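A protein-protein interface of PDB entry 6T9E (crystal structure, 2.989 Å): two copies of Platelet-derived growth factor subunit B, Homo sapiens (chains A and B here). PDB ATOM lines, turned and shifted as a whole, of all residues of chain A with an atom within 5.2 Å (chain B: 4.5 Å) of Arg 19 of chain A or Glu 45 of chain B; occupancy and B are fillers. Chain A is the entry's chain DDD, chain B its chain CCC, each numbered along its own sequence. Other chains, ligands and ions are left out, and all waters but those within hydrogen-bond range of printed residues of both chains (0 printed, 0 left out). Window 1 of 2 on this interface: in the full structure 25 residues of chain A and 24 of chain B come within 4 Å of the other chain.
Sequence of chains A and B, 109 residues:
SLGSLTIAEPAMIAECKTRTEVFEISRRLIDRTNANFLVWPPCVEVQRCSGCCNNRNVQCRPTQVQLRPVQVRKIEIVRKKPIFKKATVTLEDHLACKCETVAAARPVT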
ATOM      1  N   MET A  12      16.809  13.327  20.718  1.00  0.00           N
ATOM      2  CA  MET A  12      17.539  13.682  19.508  1.00  0.00           C
ATOM      3  C   MET A  12      18.282  12.454  18.989  1.00  0.00           C
ATOM      4  O   MET A  12      19.001  11.794  19.745  1.00  0.00           O
ATOM      5  CB  MET A  12      18.613  14.726  19.816  1.00  0.00           C
ATOM      6  CG  MET A  12      18.147  15.882  20.661  1.00  0.00           C
ATOM      7  SD  MET A  12      17.738  17.252  19.587  1.00  0.00           S
ATOM      8  CE  MET A  12      19.279  17.459  18.693  1.00  0.00           C
ATOM      9  N   ALA A  14      21.047  10.173  17.368  1.00  0.00           N
ATOM     10  CA  ALA A  14      22.480  10.189  17.176  1.00  0.00           C
ATOM     11  C   ALA A  14      22.777  10.135  15.677  1.00  0.00           C
ATOM     12  O   ALA A  14      22.526   9.115  15.024  1.00  0.00           O
ATOM     13  CB  ALA A  14      23.048   9.003  17.899  1.00  0.00           C
ATOM     14  N   GLU A  15      23.294  11.239  15.126  1.00  0.00           N
ATOM     15  CA  GLU A  15      23.489  11.248  13.687  1.00  0.00           C
ATOM     16  C   GLU A  15      24.681  10.377  13.284  1.00  0.00           C
ATOM     17  O   GLU A  15      25.554  10.049  14.080  1.00  0.00           O
ATOM     18  CB  GLU A  15      23.514  12.681  13.168  1.00  0.00           C
ATOM     19  CG  GLU A  15      24.900  13.185  12.866  1.00  0.00           C
ATOM     20  CD  GLU A  15      24.962  14.686  12.990  1.00  0.00           C
ATOM     21  OE1 GLU A  15      24.755  15.190  14.125  1.00  0.00           O
ATOM     22  OE2 GLU A  15      25.182  15.338  11.946  1.00  0.00           O
ATOM     23  N   CYS A  16      24.692   9.991  12.015  1.00  0.00           N
ATOM     24  CA  CYS A  16      25.790   9.253  11.422  1.00  0.00           C
ATOM     25  C   CYS A  16      26.960  10.197  11.158  1.00  0.00           C
ATOM     26  O   CYS A  16      26.959  10.941  10.182  1.00  0.00           O
ATOM     27  CB  CYS A  16      25.282   8.608  10.143  1.00  0.00           C
ATOM     28  SG  CYS A  16      26.495   7.591   9.272  1.00  0.00           S
ATOM     29  N   LYS A  17      27.939  10.165  12.069  1.00  0.00           N
ATOM     30  CA  LYS A  17      29.168  10.936  11.944  1.00  0.00           C
ATOM     31  C   LYS A  17      30.310  10.265  12.716  1.00  0.00           C
ATOM     32  O   LYS A  17      30.127   9.263  13.406  1.00  0.00           O
ATOM     33  CB  LYS A  17      28.961  12.394  12.376  1.00  0.00           C
ATOM     34  CG  LYS A  17      28.578  12.583  13.838  1.00  0.00           C
ATOM     35  CD  LYS A  17      28.795  13.990  14.343  1.00  0.00           C
ATOM     36  CE  LYS A  17      27.868  14.359  15.482  1.00  0.00           C
ATOM     37  NZ  LYS A  17      28.276  13.695  16.740  1.00  0.00           N
ATOM     38  N   THR A  18      31.506  10.836  12.556  1.00  0.00           N
ATOM     39  CA  THR A  18      32.716  10.334  13.173  1.00  0.00           C
ATOM     40  C   THR A  18      32.785  10.839  14.602  1.00  0.00           C
ATOM     41  O   THR A  18      32.573  12.025  14.871  1.00  0.00           O
ATOM     42  CB  THR A  18      33.927  10.865  12.410  1.00  0.00           C
ATOM     43  OG1 THR A  18      33.593  12.214  12.050  1.00  0.00           O
ATOM     44  CG2 THR A  18      34.207  10.012  11.196  1.00  0.00           C
ATOM     45  N   ARG A  19      33.121   9.912  15.498  1.00  0.00           N
ATOM     46  CA  ARG A  19      33.112  10.183  16.922  1.00  0.00           C
ATOM     47  C   ARG A  19      34.338   9.543  17.569  1.00  0.00           C
ATOM     48  O   ARG A  19      34.606   8.379  17.291  1.00  0.00           O
ATOM     49  CB  ARG A  19      31.829   9.592  17.516  1.00  0.00           C
ATOM     50  CG  ARG A  19      30.645  10.547  17.530  1.00  0.00           C
ATOM     51  CD  ARG A  19      29.473   9.855  18.193  1.00  0.00           C
ATOM     52  NE  ARG A  19      28.193  10.506  17.981  1.00  0.00           N
ATOM     53  CZ  ARG A  19      27.455  10.405  16.878  1.00  0.00           C
ATOM     54  NH1 ARG A  19      27.860   9.691  15.840  1.00  0.00           N
ATOM     55  NH2 ARG A  19      26.304  11.043  16.817  1.00  0.00           N
ATOM     56  N   THR A  20      35.030  10.297  18.445  1.00  0.00           N
ATOM     57  CA  THR A  20      36.194   9.843  19.194  1.00  0.00           C
ATOM     58  C   THR A  20      35.847   8.655  20.082  1.00  0.00           C
ATOM     59  O   THR A  20      34.918   8.722  20.863  1.00  0.00           O
ATOM     60  CB  THR A  20      36.781  10.967  20.045  1.00  0.00           C
ATOM     61  OG1 THR A  20      36.827  12.150  19.245  1.00  0.00           O
ATOM     62  CG2 THR A  20      38.150  10.598  20.565  1.00  0.00           C
ATOM     63  N   GLU A  21      36.593   7.561  19.930  1.00  0.00           N
ATOM     64  CA  GLU A  21      36.390   6.329  20.685  1.00  0.00           C
ATOM     65  C   GLU A  21      37.725   5.896  21.278  1.00  0.00           C
ATOM     66  O   GLU A  21      38.764   6.430  20.906  1.00  0.00           O
ATOM     67  CB  GLU A  21      35.795   5.208  19.833  1.00  0.00           C
ATOM     68  CG  GLU A  21      34.578   5.681  19.067  1.00  0.00           C
ATOM     69  CD  GLU A  21      33.723   4.631  18.376  1.00  0.00           C
ATOM     70  OE1 GLU A  21      33.960   3.413  18.632  1.00  0.00           O
ATOM     71  OE2 GLU A  21      32.808   5.035  17.585  1.00  0.00           O
ATOM     72  N   VAL A  46      40.757   7.023  18.769  1.00  0.00           N
ATOM     73  CA  VAL A  46      40.560   6.754  17.350  1.00  0.00           C
ATOM     74  C   VAL A  46      39.317   7.537  16.896  1.00  0.00           C
ATOM     75  O   VAL A  46      38.614   8.095  17.729  1.00  0.00           O
ATOM     76  CB  VAL A  46      40.472   5.229  17.068  1.00  0.00           C
ATOM     77  CG1 VAL A  46      41.707   4.467  17.523  1.00  0.00           C
ATOM     78  CG2 VAL A  46      39.242   4.576  17.669  1.00  0.00           C
ATOM     79  N   GLN A  47      39.071   7.641  15.582  1.00  0.00           N
ATOM     80  CA  GLN A  47      37.803   8.136  15.066  1.00  0.00           C
ATOM     81  C   GLN A  47      37.063   6.966  14.432  1.00  0.00           C
ATOM     82  O   GLN A  47      37.623   6.222  13.636  1.00  0.00           O
ATOM     83  CB  GLN A  47      37.992   9.202  13.993  1.00  0.00           C
ATOM     84  CG  GLN A  47      38.917  10.327  14.402  1.00  0.00           C
ATOM     85  CD  GLN A  47      38.194  11.295  15.298  1.00  0.00           C
ATOM     86  OE1 GLN A  47      37.239  11.945  14.876  1.00  0.00           O
ATOM     87  NE2 GLN A  47      38.658  11.410  16.536  1.00  0.00           N
ATOM     88  N   ARG A  48      35.799   6.791  14.806  1.00  0.00           N
ATOM     89  CA  ARG A  48      34.957   5.800  14.158  1.00  0.00           C
ATOM     90  C   ARG A  48      33.600   6.428  13.812  1.00  0.00           C
ATOM     91  O   ARG A  48      33.161   7.418  14.404  1.00  0.00           O
ATOM     92  CB  ARG A  48      34.878   4.505  14.980  1.00  0.00           C
ATOM     93  CG  ARG A  48      36.149   4.113  15.716  1.00  0.00           C
ATOM     94  CD  ARG A  48      37.320   3.608  14.903  1.00  0.00           C
ATOM     95  NE  ARG A  48      36.961   2.641  13.883  1.00  0.00           N
ATOM     96  CZ  ARG A  48      36.567   1.381  14.100  1.00  0.00           C
ATOM     97  NH1 ARG A  48      36.461   0.917  15.339  1.00  0.00           N
ATOM     98  NH2 ARG A  48      36.273   0.598  13.064  1.00  0.00           N
ATOM     99  N   CYS A  49      32.955   5.863  12.788  1.00  0.00           N
ATOM    100  CA  CYS A  49      31.566   6.148  12.499  1.00  0.00           C
ATOM    101  C   CYS A  49      30.706   5.448  13.540  1.00  0.00           C
ATOM    102  O   CYS A  49      30.988   4.302  13.903  1.00  0.00           O
ATOM    103  CB  CYS A  49      31.171   5.592  11.140  1.00  0.00           C
ATOM    104  SG  CYS A  49      31.873   6.536   9.769  1.00  0.00           S
ATOM    105  N   SER A  50      29.682   6.174  14.002  1.00  0.00           N
ATOM    106  CA  SER A  50      28.653   5.686  14.905  1.00  0.00           C
ATOM    107  C   SER A  50      27.443   6.570  14.702  1.00  0.00           C
ATOM    108  O   SER A  50      27.577   7.668  14.172  1.00  0.00           O
ATOM    109  CB  SER A  50      29.101   5.746  16.341  1.00  0.00           C
ATOM    110  OG  SER A  50      29.819   6.942  16.610  1.00  0.00           O
ATOM    111  N   GLY A  51      26.276   6.087  15.109  1.00  0.00           N
ATOM    112  CA  GLY A  51      25.089   6.905  14.916  1.00  0.00           C
ATOM    113  C   GLY A  51      24.040   6.216  14.052  1.00  0.00           C
ATOM    114  O   GLY A  51      24.311   5.207  13.412  1.00  0.00           O
ATOM    115  N   THR B  20      31.638  11.573  24.205  1.00  0.00           N
ATOM    116  CA  THR B  20      30.360  11.339  23.543  1.00  0.00           C
ATOM    117  C   THR B  20      30.301   9.937  22.954  1.00  0.00           C
ATOM    118  O   THR B  20      31.189   9.553  22.215  1.00  0.00           O
ATOM    119  CB  THR B  20      30.109  12.366  22.443  1.00  0.00           C
ATOM    120  OG1 THR B  20      30.394  13.649  22.995  1.00  0.00           O
ATOM    121  CG2 THR B  20      28.683  12.305  21.957  1.00  0.00           C
ATOM    122  N   GLU B  21      29.267   9.174  23.318  1.00  0.00           N
ATOM    123  CA  GLU B  21      29.074   7.806  22.854  1.00  0.00           C
ATOM    124  C   GLU B  21      27.656   7.668  22.313  1.00  0.00           C
ATOM    125  O   GLU B  21      26.830   8.549  22.532  1.00  0.00           O
ATOM    126  CB  GLU B  21      29.323   6.792  23.968  1.00  0.00           C
ATOM    127  CG  GLU B  21      30.662   7.015  24.635  1.00  0.00           C
ATOM    128  CD  GLU B  21      31.199   5.922  25.541  1.00  0.00           C
ATOM    129  OE1 GLU B  21      30.629   4.808  25.522  1.00  0.00           O
ATOM    130  OE2 GLU B  21      32.202   6.186  26.257  1.00  0.00           O
ATOM    131  N   VAL B  22      27.392   6.582  21.574  1.00  0.00           N
ATOM    132  CA  VAL B  22      26.083   6.376  20.979  1.00  0.00           C
ATOM    133  C   VAL B  22      25.408   5.216  21.698  1.00  0.00           C
ATOM    134  O   VAL B  22      25.920   4.100  21.664  1.00  0.00           O
ATOM    135  CB  VAL B  22      26.187   6.100  19.471  1.00  0.00           C
ATOM    136  CG1 VAL B  22      25.068   5.206  18.975  1.00  0.00           C
ATOM    137  CG2 VAL B  22      26.244   7.381  18.659  1.00  0.00           C
ATOM    138  N   VAL B  44      20.575   7.468  20.775  1.00  0.00           N
ATOM    139  CA  VAL B  44      20.853   8.817  21.246  1.00  0.00           C
ATOM    140  C   VAL B  44      22.312   8.909  21.701  1.00  0.00           C
ATOM    141  O   VAL B  44      22.894   7.908  22.134  1.00  0.00           O
ATOM    142  CB  VAL B  44      19.919   9.174  22.421  1.00  0.00           C
ATOM    143  CG1 VAL B  44      19.983  10.651  22.790  1.00  0.00           C
ATOM    144  CG2 VAL B  44      18.487   8.734  22.166  1.00  0.00           C
ATOM    145  N   GLU B  45      22.869  10.133  21.631  1.00  0.00           N
ATOM    146  CA  GLU B  45      24.167  10.464  22.200  1.00  0.00           C
ATOM    147  C   GLU B  45      24.079  10.558  23.724  1.00  0.00           C
ATOM    148  O   GLU B  45      23.073  10.993  24.271  1.00  0.00           O
ATOM    149  CB  GLU B  45      24.634  11.807  21.647  1.00  0.00           C
ATOM    150  CG  GLU B  45      25.523  11.690  20.430  1.00  0.00           C
ATOM    151  CD  GLU B  45      25.950  13.033  19.856  1.00  0.00           C
ATOM    152  OE1 GLU B  45      25.244  14.036  20.127  1.00  0.00           O
ATOM    153  OE2 GLU B  45      26.993  13.080  19.149  1.00  0.00           O
ATOM    154  N   VAL B  46      25.166  10.168  24.397  1.00  0.00           N
ATOM    155  CA  VAL B  46      25.308  10.170  25.847  1.00  0.00           C
ATOM    156  C   VAL B  46      26.744  10.610  26.176  1.00  0.00           C
ATOM    157  O   VAL B  46      27.560  10.726  25.272  1.00  0.00           O
ATOM    158  CB  VAL B  46      24.931   8.786  26.447  1.00  0.00           C
ATOM    159  CG1 VAL B  46      23.505   8.357  26.124  1.00  0.00           C
ATOM    160  CG2 VAL B  46      25.891   7.671  26.056  1.00  0.00           C
ATOM    161  N   ARG B  68      19.053  11.974  32.951  1.00  0.00           N
ATOM    162  CA  ARG B  68      18.427  12.787  31.918  1.00  0.00           C
ATOM    163  C   ARG B  68      17.329  11.960  31.256  1.00  0.00           C
ATOM    164  O   ARG B  68      17.616  11.068  30.455  1.00  0.00           O
ATOM    165  CB  ARG B  68      19.439  13.251  30.867  1.00  0.00           C
ATOM    166  CG  ARG B  68      18.799  13.978  29.698  1.00  0.00           C
ATOM    167  CD  ARG B  68      19.767  14.347  28.595  1.00  0.00           C
ATOM    168  NE  ARG B  68      20.781  13.348  28.284  1.00  0.00           N
ATOM    169  CZ  ARG B  68      21.413  13.252  27.115  1.00  0.00           C
ATOM    170  NH1 ARG B  68      21.110  14.082  26.127  1.00  0.00           N
ATOM    171  NH2 ARG B  68      22.326  12.312  26.923  1.00  0.00           N
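The guanidinium group (NE) of Arg 19 of chain A lies within salt-bridge range of the side-chain carboxylate (OE2) of Glu 45 of chain B. NZ of Lys 17 of chain A lies within salt-bridge range of OE2 of Glu 45 of chain B.
The guanidinium group (NH1) of Arg 19 of chain A lies within hydrogen-bond range of the backbone carbonyl oxygen (O) of Ser 50 of chain A (2.6 Å). NH2 of Arg 68 of chain B lies within hydrogen-bond range of O of Glu 45 of chain B (3.1 Å). The backbone carbonyl oxygen of Lys 17 of chain A sits at hydrogen-bond distance from the guanidinium group of Arg 19 of chain A (3.4 Å). NH1 of Arg 19 of chain A is in hydrogen-bond range of O of Glu 15 of chain A. The backbone NH (N) of Arg 19 of chain A sits at hydrogen-bond distance from the backbone carbonyl oxygen (O) of Arg 48 of chain A. The backbone NH of Ser 50 of chain A lies within hydrogen-bond range of the backbone carbonyl oxygen of Lys 17 of chain A.
Among the printed residues, merely in contact across the chains: Met 12 of chain A with Val 44 of chain B, Ala 14 of chain A with Val 22 of chain B, Arg 19 of chain A with Val 22 of chain B, Gly 51 of chain A with Val 22 of chain B, Ala 14 of chain A with Val 44 of chain B and Ala 14 of chain A with Glu 45 of chain B.
Arg 19 of chain A touches just these residues of chain B: Val 22 (3.7 Å) and Glu 45 (3.1 Å). Glu 45 of chain B touches just these residues of chain A: Ala 14 (3.9 Å), Lys 17 (2.8 Å) and Arg 19 (3.1 Å). Of the printed residues of chain A, Val 22 of chain B touches Ala 14 (3.7 Å), Arg 19 (3.7 Å) and Gly 51 (3.8 Å). Printed residues of chain B within 4 Å of Gly 51 of chain A: Val 22 (3.8 Å). Of the printed residues of chain B, Ala 14 of chain A touches Val 22, Val 44 and Glu 45. Of the printed residues of chain B, Lys 17 of chain A touches Glu 45. The nearest residue of chain B that does not touch Arg 19 of chain A is Thr 20 of chain B (4.4 Å).
Of the 7 printed residues of chain B, 3 touch a printed residue of chain A. Hydrophobic or aromatic side chains of chain B within 4 Å of the printed part of chain A: Val 22 and Val 44. Along chain B the printed residues that touch a printed residue of chain A span positions 22 to 45. Among the printed residues, Asp or Glu carboxylates within 4 Å of a Lys or Arg side-chain nitrogen of the other chain: Lys 17 of chain A with Glu 45 of chain B (2.8 Å) and Arg 19 of chain A with Glu 45 of chain B (3.1 Å).
Positions printed for both chains: 20, 21 and 46. Of the 8 pairs that touch across the chains among the printed residues, none has its exchanged pair printed and touching as well.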
